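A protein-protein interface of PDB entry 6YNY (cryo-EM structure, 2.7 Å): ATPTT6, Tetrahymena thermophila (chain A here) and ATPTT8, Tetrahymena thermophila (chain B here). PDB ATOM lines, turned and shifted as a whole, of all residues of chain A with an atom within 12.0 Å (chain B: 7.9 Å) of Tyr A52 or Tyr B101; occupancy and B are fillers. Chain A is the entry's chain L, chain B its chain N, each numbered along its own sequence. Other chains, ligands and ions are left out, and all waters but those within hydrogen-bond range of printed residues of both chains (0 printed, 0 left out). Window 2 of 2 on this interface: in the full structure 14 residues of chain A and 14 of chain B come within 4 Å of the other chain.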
ATOM      1  N   ASN A  46      11.783 -26.002 -10.337  1.00  0.00           N
ATOM      2  CA  ASN A  46      12.579 -24.785 -10.413  1.00  0.00           C
ATOM      3  C   ASN A  46      12.911 -24.329  -8.999  1.00  0.00           C
ATOM      4  O   ASN A  46      12.012 -24.006  -8.215  1.00  0.00           O
ATOM      5  CB  ASN A  46      11.830 -23.698 -11.179  1.00  0.00           C
ATOM      6  CG  ASN A  46      10.536 -23.295 -10.506  1.00  0.00           C
ATOM      7  OD1 ASN A  46       9.520 -23.978 -10.624  1.00  0.00           O
ATOM      8  ND2 ASN A  46      10.566 -22.173  -9.797  1.00  0.00           N
ATOM      9  N   ARG A  47      14.196 -24.316  -8.670  1.00  0.00           N
ATOM     10  CA  ARG A  47      14.618 -23.967  -7.325  1.00  0.00           C
ATOM     11  C   ARG A  47      14.454 -22.474  -7.081  1.00  0.00           C
ATOM     12  O   ARG A  47      14.770 -21.648  -7.940  1.00  0.00           O
ATOM     13  CB  ARG A  47      16.076 -24.366  -7.113  1.00  0.00           C
ATOM     14  CG  ARG A  47      16.416 -25.784  -7.534  1.00  0.00           C
ATOM     15  CD  ARG A  47      16.581 -26.701  -6.361  1.00  0.00           C
ATOM     16  NE  ARG A  47      17.100 -28.003  -6.762  1.00  0.00           N
ATOM     17  CZ  ARG A  47      18.392 -28.282  -6.896  1.00  0.00           C
ATOM     18  NH1 ARG A  47      18.776 -29.494  -7.263  1.00  0.00           N
ATOM     19  NH2 ARG A  47      19.305 -27.352  -6.670  1.00  0.00           N
ATOM     20  N   LYS A  48      13.945 -22.128  -5.903  1.00  0.00           N
ATOM     21  CA  LYS A  48      13.911 -20.738  -5.485  1.00  0.00           C
ATOM     22  C   LYS A  48      15.301 -20.292  -5.056  1.00  0.00           C
ATOM     23  O   LYS A  48      16.122 -21.096  -4.609  1.00  0.00           O
ATOM     24  CB  LYS A  48      12.930 -20.534  -4.334  1.00  0.00           C
ATOM     25  CG  LYS A  48      11.482 -20.737  -4.703  1.00  0.00           C
ATOM     26  CD  LYS A  48      10.578 -20.382  -3.541  1.00  0.00           C
ATOM     27  CE  LYS A  48       9.129 -20.731  -3.822  1.00  0.00           C
ATOM     28  NZ  LYS A  48       8.597 -20.054  -5.035  1.00  0.00           N
ATOM     29  N   THR A  49      15.560 -18.993  -5.193  1.00  0.00           N
ATOM     30  CA  THR A  49      16.867 -18.427  -4.896  1.00  0.00           C
ATOM     31  C   THR A  49      16.845 -17.525  -3.669  1.00  0.00           C
ATOM     32  O   THR A  49      17.782 -16.750  -3.455  1.00  0.00           O
ATOM     33  CB  THR A  49      17.396 -17.660  -6.106  1.00  0.00           C
ATOM     34  OG1 THR A  49      16.482 -16.610  -6.447  1.00  0.00           O
ATOM     35  CG2 THR A  49      17.550 -18.597  -7.279  1.00  0.00           C
ATOM     36  N   GLN A  50      15.792 -17.603  -2.862  1.00  0.00           N
ATOM     37  CA  GLN A  50      15.710 -16.848  -1.621  1.00  0.00           C
ATOM     38  C   GLN A  50      15.185 -17.763  -0.529  1.00  0.00           C
ATOM     39  O   GLN A  50      14.205 -18.485  -0.735  1.00  0.00           O
ATOM     40  CB  GLN A  50      14.813 -15.618  -1.764  1.00  0.00           C
ATOM     41  CG  GLN A  50      14.661 -14.818  -0.484  1.00  0.00           C
ATOM     42  CD  GLN A  50      15.990 -14.411   0.121  1.00  0.00           C
ATOM     43  OE1 GLN A  50      16.164 -14.442   1.339  1.00  0.00           O
ATOM     44  NE2 GLN A  50      16.933 -14.022  -0.727  1.00  0.00           N
ATOM     45  N   GLU A  51      15.838 -17.726   0.625  1.00  0.00           N
ATOM     46  CA  GLU A  51      15.505 -18.600   1.735  1.00  0.00           C
ATOM     47  C   GLU A  51      14.432 -17.961   2.605  1.00  0.00           C
ATOM     48  O   GLU A  51      14.478 -16.761   2.890  1.00  0.00           O
ATOM     49  CB  GLU A  51      16.760 -18.891   2.555  1.00  0.00           C
ATOM     50  CG  GLU A  51      16.580 -19.859   3.687  1.00  0.00           C
ATOM     51  CD  GLU A  51      17.886 -20.154   4.392  1.00  0.00           C
ATOM     52  OE1 GLU A  51      18.910 -20.324   3.699  1.00  0.00           O
ATOM     53  OE2 GLU A  51      17.895 -20.202   5.639  1.00  0.00           O
ATOM     54  N   TYR A  52      13.462 -18.770   3.016  1.00  0.00           N
ATOM     55  CA  TYR A  52      12.371 -18.305   3.856  1.00  0.00           C
ATOM     56  C   TYR A  52      12.767 -18.369   5.322  1.00  0.00           C
ATOM     57  O   TYR A  52      13.443 -19.304   5.757  1.00  0.00           O
ATOM     58  CB  TYR A  52      11.113 -19.139   3.621  1.00  0.00           C
ATOM     59  CG  TYR A  52       9.947 -18.732   4.486  1.00  0.00           C
ATOM     60  CD1 TYR A  52       9.160 -17.644   4.152  1.00  0.00           C
ATOM     61  CD2 TYR A  52       9.633 -19.437   5.637  1.00  0.00           C
ATOM     62  CE1 TYR A  52       8.096 -17.267   4.938  1.00  0.00           C
ATOM     63  CE2 TYR A  52       8.571 -19.067   6.430  1.00  0.00           C
ATOM     64  CZ  TYR A  52       7.805 -17.981   6.077  1.00  0.00           C
ATOM     65  OH  TYR A  52       6.744 -17.606   6.864  1.00  0.00           O
ATOM     66  N   PHE A  53      12.342 -17.364   6.081  1.00  0.00           N
ATOM     67  CA  PHE A  53      12.661 -17.259   7.495  1.00  0.00           C
ATOM     68  C   PHE A  53      11.376 -17.040   8.274  1.00  0.00           C
ATOM     69  O   PHE A  53      10.610 -16.122   7.972  1.00  0.00           O
ATOM     70  CB  PHE A  53      13.640 -16.117   7.762  1.00  0.00           C
ATOM     71  CG  PHE A  53      14.913 -16.220   6.984  1.00  0.00           C
ATOM     72  CD1 PHE A  53      15.111 -15.448   5.857  1.00  0.00           C
ATOM     73  CD2 PHE A  53      15.910 -17.093   7.372  1.00  0.00           C
ATOM     74  CE1 PHE A  53      16.277 -15.541   5.138  1.00  0.00           C
ATOM     75  CE2 PHE A  53      17.077 -17.189   6.653  1.00  0.00           C
ATOM     76  CZ  PHE A  53      17.260 -16.413   5.536  1.00  0.00           C
ATOM     77  N   LEU A  54      11.147 -17.887   9.271  1.00  0.00           N
ATOM     78  CA  LEU A  54       9.961 -17.782  10.108  1.00  0.00           C
ATOM     79  C   LEU A  54      10.162 -16.690  11.148  1.00  0.00           C
ATOM     80  O   LEU A  54      11.076 -16.770  11.974  1.00  0.00           O
ATOM     81  CB  LEU A  54       9.677 -19.119  10.781  1.00  0.00           C
ATOM     82  CG  LEU A  54       8.461 -19.168  11.698  1.00  0.00           C
ATOM     83  CD1 LEU A  54       7.195 -18.864  10.928  1.00  0.00           C
ATOM     84  CD2 LEU A  54       8.379 -20.518  12.351  1.00  0.00           C
ATOM     85  N   GLU A  55       9.307 -15.676  11.109  1.00  0.00           N
ATOM     86  CA  GLU A  55       9.368 -14.562  12.037  1.00  0.00           C
ATOM     87  C   GLU A  55       7.981 -14.251  12.572  1.00  0.00           C
ATOM     88  O   GLU A  55       6.978 -14.534  11.910  1.00  0.00           O
ATOM     89  CB  GLU A  55       9.937 -13.308  11.361  1.00  0.00           C
ATOM     90  CG  GLU A  55      11.328 -13.479  10.805  1.00  0.00           C
ATOM     91  CD  GLU A  55      11.863 -12.207  10.181  1.00  0.00           C
ATOM     92  OE1 GLU A  55      11.133 -11.193  10.181  1.00  0.00           O
ATOM     93  OE2 GLU A  55      13.010 -12.218   9.691  1.00  0.00           O
ATOM     94  N   PRO A  56       7.892 -13.676  13.770  1.00  0.00           N
ATOM     95  CA  PRO A  56       6.586 -13.253  14.284  1.00  0.00           C
ATOM     96  C   PRO A  56       6.101 -12.005  13.565  1.00  0.00           C
ATOM     97  O   PRO A  56       6.798 -10.989  13.513  1.00  0.00           O
ATOM     98  CB  PRO A  56       6.858 -12.989  15.767  1.00  0.00           C
ATOM     99  CG  PRO A  56       8.287 -12.666  15.831  1.00  0.00           C
ATOM    100  CD  PRO A  56       8.961 -13.461  14.759  1.00  0.00           C
ATOM    101  N   SER A  57       4.897 -12.086  13.009  1.00  0.00           N
ATOM    102  CA  SER A  57       4.338 -10.977  12.258  1.00  0.00           C
ATOM    103  C   SER A  57       3.884  -9.868  13.204  1.00  0.00           C
ATOM    104  O   SER A  57       4.065  -9.931  14.423  1.00  0.00           O
ATOM    105  CB  SER A  57       3.178 -11.461  11.393  1.00  0.00           C
ATOM    106  OG  SER A  57       2.167 -12.051  12.188  1.00  0.00           O
ATOM    107  N   GLU A  58       3.286  -8.827  12.621  1.00  0.00           N
ATOM    108  CA  GLU A  58       2.756  -7.733  13.426  1.00  0.00           C
ATOM    109  C   GLU A  58       1.473  -8.144  14.134  1.00  0.00           C
ATOM    110  O   GLU A  58       1.236  -7.751  15.280  1.00  0.00           O
ATOM    111  CB  GLU A  58       2.509  -6.509  12.547  1.00  0.00           C
ATOM    112  CG  GLU A  58       3.685  -6.106  11.668  1.00  0.00           C
ATOM    113  CD  GLU A  58       4.862  -5.556  12.457  1.00  0.00           C
ATOM    114  OE1 GLU A  58       5.063  -5.975  13.616  1.00  0.00           O
ATOM    115  OE2 GLU A  58       5.590  -4.701  11.912  1.00  0.00           O
ATOM    116  N   PHE A  60       1.065 -10.994  15.198  1.00  0.00           N
ATOM    117  CA  PHE A  60       1.595 -11.811  16.280  1.00  0.00           C
ATOM    118  C   PHE A  60       1.989 -10.949  17.471  1.00  0.00           C
ATOM    119  O   PHE A  60       1.534 -11.177  18.595  1.00  0.00           O
ATOM    120  CB  PHE A  60       2.791 -12.604  15.761  1.00  0.00           C
ATOM    121  CG  PHE A  60       3.347 -13.594  16.734  1.00  0.00           C
ATOM    122  CD1 PHE A  60       4.209 -13.196  17.733  1.00  0.00           C
ATOM    123  CD2 PHE A  60       3.038 -14.933  16.623  1.00  0.00           C
ATOM    124  CE1 PHE A  60       4.729 -14.108  18.615  1.00  0.00           C
ATOM    125  CE2 PHE A  60       3.558 -15.846  17.502  1.00  0.00           C
ATOM    126  CZ  PHE A  60       4.405 -15.435  18.497  1.00  0.00           C
ATOM    127  N   LEU B  91       1.015 -31.660  11.290  1.00  0.00           N
ATOM    128  CA  LEU B  91       1.425 -30.571  10.420  1.00  0.00           C
ATOM    129  C   LEU B  91       0.548 -30.464   9.184  1.00  0.00           C
ATOM    130  O   LEU B  91       0.474 -29.388   8.582  1.00  0.00           O
ATOM    131  CB  LEU B  91       2.882 -30.767  10.015  1.00  0.00           C
ATOM    132  CG  LEU B  91       3.550 -29.611   9.280  1.00  0.00           C
ATOM    133  CD1 LEU B  91       3.604 -28.385  10.165  1.00  0.00           C
ATOM    134  CD2 LEU B  91       4.935 -30.022   8.849  1.00  0.00           C
ATOM    135  N   ASP B  97      -1.754 -22.014   4.010  1.00  0.00           N
ATOM    136  CA  ASP B  97      -0.484 -22.279   3.356  1.00  0.00           C
ATOM    137  C   ASP B  97       0.664 -21.793   4.229  1.00  0.00           C
ATOM    138  O   ASP B  97       0.580 -20.735   4.857  1.00  0.00           O
ATOM    139  CB  ASP B  97      -0.426 -21.591   1.992  1.00  0.00           C
ATOM    140  CG  ASP B  97      -1.588 -21.973   1.097  1.00  0.00           C
ATOM    141  OD1 ASP B  97      -2.723 -21.533   1.377  1.00  0.00           O
ATOM    142  OD2 ASP B  97      -1.366 -22.712   0.116  1.00  0.00           O
ATOM    143  N   PHE B  98       1.738 -22.574   4.256  1.00  0.00           N
ATOM    144  CA  PHE B  98       2.895 -22.252   5.076  1.00  0.00           C
ATOM    145  C   PHE B  98       4.107 -22.951   4.485  1.00  0.00           C
ATOM    146  O   PHE B  98       3.982 -23.910   3.719  1.00  0.00           O
ATOM    147  CB  PHE B  98       2.684 -22.672   6.532  1.00  0.00           C
ATOM    148  CG  PHE B  98       2.490 -24.144   6.710  1.00  0.00           C
ATOM    149  CD1 PHE B  98       3.552 -24.954   7.048  1.00  0.00           C
ATOM    150  CD2 PHE B  98       1.249 -24.720   6.528  1.00  0.00           C
ATOM    151  CE1 PHE B  98       3.382 -26.306   7.206  1.00  0.00           C
ATOM    152  CE2 PHE B  98       1.073 -26.073   6.686  1.00  0.00           C
ATOM    153  CZ  PHE B  98       2.140 -26.868   7.025  1.00  0.00           C
ATOM    154  N   VAL B  99       5.284 -22.456   4.853  1.00  0.00           N
ATOM    155  CA  VAL B  99       6.554 -23.001   4.390  1.00  0.00           C
ATOM    156  C   VAL B  99       7.244 -23.656   5.574  1.00  0.00           C
ATOM    157  O   VAL B  99       7.500 -23.003   6.593  1.00  0.00           O
ATOM    158  CB  VAL B  99       7.444 -21.916   3.770  1.00  0.00           C
ATOM    159  CG1 VAL B  99       8.684 -22.538   3.171  1.00  0.00           C
ATOM    160  CG2 VAL B  99       6.679 -21.137   2.728  1.00  0.00           C
ATOM    161  N   GLU B 100       7.548 -24.943   5.438  1.00  0.00           N
ATOM    162  CA  GLU B 100       8.246 -25.694   6.468  1.00  0.00           C
ATOM    163  C   GLU B 100       9.331 -26.531   5.816  1.00  0.00           C
ATOM    164  O   GLU B 100       9.072 -27.235   4.836  1.00  0.00           O
ATOM    165  CB  GLU B 100       7.285 -26.594   7.252  1.00  0.00           C
ATOM    166  CG  GLU B 100       6.776 -25.980   8.541  1.00  0.00           C
ATOM    167  CD  GLU B 100       7.870 -25.791   9.567  1.00  0.00           C
ATOM    168  OE1 GLU B 100       8.965 -26.360   9.382  1.00  0.00           O
ATOM    169  OE2 GLU B 100       7.637 -25.071  10.559  1.00  0.00           O
ATOM    170  N   TYR B 101      10.539 -26.446   6.359  1.00  0.00           N
ATOM    171  CA  TYR B 101      11.660 -27.220   5.859  1.00  0.00           C
ATOM    172  C   TYR B 101      11.781 -28.521   6.636  1.00  0.00           C
ATOM    173  O   TYR B 101      11.619 -28.548   7.859  1.00  0.00           O
ATOM    174  CB  TYR B 101      12.958 -26.422   5.970  1.00  0.00           C
ATOM    175  CG  TYR B 101      12.984 -25.168   5.133  1.00  0.00           C
ATOM    176  CD1 TYR B 101      12.993 -25.235   3.752  1.00  0.00           C
ATOM    177  CD2 TYR B 101      13.017 -23.919   5.725  1.00  0.00           C
ATOM    178  CE1 TYR B 101      13.020 -24.094   2.987  1.00  0.00           C
ATOM    179  CE2 TYR B 101      13.046 -22.775   4.967  1.00  0.00           C
ATOM    180  CZ  TYR B 101      13.051 -22.867   3.599  1.00  0.00           C
ATOM    181  OH  TYR B 101      13.080 -21.727   2.837  1.00  0.00           O
ATOM    182  N   LYS B 102      12.069 -29.602   5.915  1.00  0.00           N
ATOM    183  CA  LYS B 102      12.184 -30.915   6.532  1.00  0.00           C
ATOM    184  C   LYS B 102      13.363 -31.014   7.486  1.00  0.00           C
ATOM    185  O   LYS B 102      13.442 -31.983   8.247  1.00  0.00           O
ATOM    186  CB  LYS B 102      12.321 -31.987   5.455  1.00  0.00           C
ATOM    187  CG  LYS B 102      11.215 -31.986   4.421  1.00  0.00           C
ATOM    188  CD  LYS B 102       9.902 -32.436   5.008  1.00  0.00           C
ATOM    189  CE  LYS B 102       8.859 -32.616   3.929  1.00  0.00           C
ATOM    190  NZ  LYS B 102       7.543 -33.004   4.480  1.00  0.00           N
ATOM    191  N   ALA B 103      14.278 -30.051   7.459  1.00  0.00           N
ATOM    192  CA  ALA B 103      15.461 -30.086   8.305  1.00  0.00           C
ATOM    193  C   ALA B 103      15.189 -29.635   9.732  1.00  0.00           C
ATOM    194  O   ALA B 103      16.109 -29.655  10.553  1.00  0.00           O
ATOM    195  CB  ALA B 103      16.555 -29.212   7.696  1.00  0.00           C
ATOM    196  N   HIS B 104      13.961 -29.231  10.046  1.00  0.00           N
ATOM    197  CA  HIS B 104      13.626 -28.713  11.362  1.00  0.00           C
ATOM    198  C   HIS B 104      12.524 -29.498  12.050  1.00  0.00           C
ATOM    199  O   HIS B 104      12.112 -29.121  13.152  1.00  0.00           O
ATOM    200  CB  HIS B 104      13.204 -27.244  11.254  1.00  0.00           C
ATOM    201  CG  HIS B 104      14.203 -26.377  10.560  1.00  0.00           C
ATOM    202  ND1 HIS B 104      13.850 -25.222   9.898  1.00  0.00           N
ATOM    203  CD2 HIS B 104      15.545 -26.490  10.429  1.00  0.00           C
ATOM    204  CE1 HIS B 104      14.930 -24.664   9.385  1.00  0.00           C
ATOM    205  NE2 HIS B 104      15.972 -25.413   9.692  1.00  0.00           N
ATOM    206  N   GLN B 105      12.040 -30.579  11.445  1.00  0.00           N
ATOM    207  CA  GLN B 105      10.881 -31.286  11.966  1.00  0.00           C
ATOM    208  C   GLN B 105      11.236 -32.411  12.924  1.00  0.00           C
ATOM    209  O   GLN B 105      10.367 -32.855  13.681  1.00  0.00           O
ATOM    210  CB  GLN B 105      10.054 -31.848  10.809  1.00  0.00           C
ATOM    211  CG  GLN B 105      10.745 -32.925  10.016  1.00  0.00           C
ATOM    212  CD  GLN B 105       9.914 -33.397   8.850  1.00  0.00           C
ATOM    213  OE1 GLN B 105       8.887 -32.805   8.525  1.00  0.00           O
ATOM    214  NE2 GLN B 105      10.350 -34.472   8.216  1.00  0.00           N
ATOM    215  N   LEU B 106      12.481 -32.879  12.919  1.00  0.00           N
ATOM    216  CA  LEU B 106      12.867 -33.986  13.781  1.00  0.00           C
ATOM    217  C   LEU B 106      13.373 -33.538  15.140  1.00  0.00           C
ATOM    218  O   LEU B 106      13.179 -34.255  16.128  1.00  0.00           O
ATOM    219  CB  LEU B 106      13.943 -34.834  13.104  1.00  0.00           C
ATOM    220  CG  LEU B 106      13.520 -35.585  11.846  1.00  0.00           C
ATOM    221  CD1 LEU B 106      14.653 -36.459  11.361  1.00  0.00           C
ATOM    222  CD2 LEU B 106      12.278 -36.411  12.096  1.00  0.00           C
ATOM    223  N   HIS B 110      10.505 -28.692  18.504  1.00  0.00           N
ATOM    224  CA  HIS B 110      10.618 -27.491  17.688  1.00  0.00           C
ATOM    225  C   HIS B 110       9.534 -27.418  16.625  1.00  0.00           C
ATOM    226  O   HIS B 110       9.074 -26.322  16.293  1.00  0.00           O
ATOM    227  CB  HIS B 110      11.997 -27.431  17.037  1.00  0.00           C
ATOM    228  CG  HIS B 110      12.277 -26.140  16.338  1.00  0.00           C
ATOM    229  ND1 HIS B 110      12.121 -24.917  16.950  1.00  0.00           N
ATOM    230  CD2 HIS B 110      12.699 -25.879  15.080  1.00  0.00           C
ATOM    231  CE1 HIS B 110      12.434 -23.958  16.099  1.00  0.00           C
ATOM    232  NE2 HIS B 110      12.788 -24.515  14.956  1.00  0.00           N
ATOM    233  N   LEU B 111       9.118 -28.560  16.083  1.00  0.00           N
ATOM    234  CA  LEU B 111       8.034 -28.562  15.109  1.00  0.00           C
ATOM    235  C   LEU B 111       6.766 -27.968  15.707  1.00  0.00           C
ATOM    236  O   LEU B 111       6.121 -27.110  15.097  1.00  0.00           O
ATOM    237  CB  LEU B 111       7.784 -29.985  14.624  1.00  0.00           C
ATOM    238  CG  LEU B 111       6.741 -30.164  13.527  1.00  0.00           C
ATOM    239  CD1 LEU B 111       7.214 -29.559  12.232  1.00  0.00           C
ATOM    240  CD2 LEU B 111       6.428 -31.627  13.348  1.00  0.00           C
ATOM    241  N   ARG B 114       7.159 -24.160  15.824  1.00  0.00           N
ATOM    242  CA  ARG B 114       6.974 -23.459  14.560  1.00  0.00           C
ATOM    243  C   ARG B 114       5.513 -23.461  14.137  1.00  0.00           C
ATOM    244  O   ARG B 114       5.009 -22.461  13.615  1.00  0.00           O
ATOM    245  CB  ARG B 114       7.845 -24.100  13.485  1.00  0.00           C
ATOM    246  CG  ARG B 114       9.314 -24.096  13.813  1.00  0.00           C
ATOM    247  CD  ARG B 114      10.126 -24.810  12.757  1.00  0.00           C
ATOM    248  NE  ARG B 114      10.104 -24.113  11.478  1.00  0.00           N
ATOM    249  CZ  ARG B 114      10.908 -23.106  11.156  1.00  0.00           C
ATOM    250  NH1 ARG B 114      11.808 -22.660  12.020  1.00  0.00           N
ATOM    251  NH2 ARG B 114      10.810 -22.538   9.966  1.00  0.00           N
ATOM    252  N   ILE B 117       3.677 -20.800  15.864  1.00  0.00           N
ATOM    253  CA  ILE B 117       3.971 -19.500  15.272  1.00  0.00           C
ATOM    254  C   ILE B 117       3.167 -19.304  13.995  1.00  0.00           C
ATOM    255  O   ILE B 117       2.532 -18.262  13.796  1.00  0.00           O
ATOM    256  CB  ILE B 117       5.480 -19.368  15.012  1.00  0.00           C
ATOM    257  CG1 ILE B 117       6.256 -19.500  16.319  1.00  0.00           C
ATOM    258  CG2 ILE B 117       5.791 -18.043  14.360  1.00  0.00           C
ATOM    259  CD1 ILE B 117       7.735 -19.642  16.133  1.00  0.00           C
ATOM    260  N   HIS B 118       3.190 -20.296  13.106  1.00  0.00           N
ATOM    261  CA  HIS B 118       2.408 -20.211  11.880  1.00  0.00           C
ATOM    262  C   HIS B 118       0.941 -19.936  12.177  1.00  0.00           C
ATOM    263  O   HIS B 118       0.295 -19.145  11.483  1.00  0.00           O
ATOM    264  CB  HIS B 118       2.551 -21.503  11.080  1.00  0.00           C
ATOM    265  CG  HIS B 118       3.876 -21.659  10.406  1.00  0.00           C
ATOM    266  ND1 HIS B 118       4.679 -22.762  10.595  1.00  0.00           N
ATOM    267  CD2 HIS B 118       4.530 -20.862   9.528  1.00  0.00           C
ATOM    268  CE1 HIS B 118       5.776 -22.632   9.873  1.00  0.00           C
ATOM    269  NE2 HIS B 118       5.711 -21.488   9.216  1.00  0.00           N
ATOM    270  N   ASN B 121       0.410 -16.362  13.436  1.00  0.00           N
ATOM    271  CA  ASN B 121       0.552 -15.356  12.395  1.00  0.00           C
ATOM    272  C   ASN B 121      -0.683 -15.300  11.504  1.00  0.00           C
ATOM    273  O   ASN B 121      -1.245 -14.225  11.281  1.00  0.00           O
ATOM    274  CB  ASN B 121       1.793 -15.638  11.550  1.00  0.00           C
ATOM    275  CG  ASN B 121       3.074 -15.359  12.290  1.00  0.00           C
ATOM    276  OD1 ASN B 121       3.097 -14.597  13.252  1.00  0.00           O
ATOM    277  ND2 ASN B 121       4.155 -15.968  11.838  1.00  0.00           N
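The backbone carbonyl oxygen (O) of Ile B117 sits close to the side-chain amide nitrogen (ND2) of Asn B121 (3.4 Å).
NE of Arg B114 is in salt-bridge range of OE2 of Glu B100, at 2.8 Å.
OG of Ser A57 is in hydrogen-bond range of N of Phe A60 (3.4 Å).
O of Arg B114 lies within hydrogen-bond range of ND1 of His B118 (3.1 Å).
Among the printed residues, pairs that only touch across the chains: Phe A60 with Asn B121 (3.2 Å), Leu A54 with His B118 (3.5 Å), Leu A54 with Arg B114 (3.7 Å), Tyr A52 with Val B99 (3.8 Å), Leu A54 with Ile B117 (3.8 Å) and Pro A56 with Asn B121 (3.9 Å).
The side-chain amide oxygen of Asn B121 sits at hydrogen-bond distance from the side-chain hydroxyl of Ser A57, 2.9 Å away.
The backbone NH of Tyr A52 lies within hydrogen-bond range of the side-chain hydroxyl of Tyr B101, 3.0 Å away.
The side-chain amide nitrogen of Asn B121 lies within hydrogen-bond range of the backbone carbonyl oxygen of Glu A55, 3.2 Å away.
Tyr A52 touches two residues of chain B.
Of the printed residues of chain A, Tyr B101 touches Tyr A52.
No residue of chain A comes within 4 Å of Glu B100.
No residue of chain A comes within 4 Å of Lys B102.
No residue of chain A comes within 4 Å of Ala B103.
His B104 touches none of the printed residues of chain A.
No residue of chain A comes within 4 Å of Gln B105.
Printed residues of chain A within 4 Å of Asn B121: Glu A55 (3.2 Å), Pro A56 (3.9 Å), Ser A57 (2.9 Å) and Phe A60 (3.2 Å).
Printed residues of chain B within 4 Å of Leu A54: Arg B114 (3.7 Å), Ile B117 (3.8 Å) and His B118 (3.5 Å).
Of the printed residues of chain B, Ser A57 touches Asn B121.
Leu B106 touches none of the printed residues of chain A.
The nearest printed residue of chain A that does not touch Tyr B101 is Glu A51 (4.01 Å).
Of the 14 printed residues of chain A, 6 touch a printed residue of chain B.
Printed residues of chain A that touch a printed residue of chain B: Tyr A52, Leu A54, Glu A55, Pro A56, Ser A57 and Phe A60.
Hydrophobic or aromatic side chains of chain A that line the printed part of chain B: Tyr A52, Leu A54 and Phe A60.
Hydrophobic or aromatic side chains of chain B within 4 Å of the printed part of chain A: Val B99, Tyr B101, Ile B117 and His B118.
Among the printed residues, 9 pairs touch across the chains.
Among the printed residues, no Asp or Glu carboxylate lies within 4 Å of a Lys or Arg side-chain nitrogen of the other chain.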
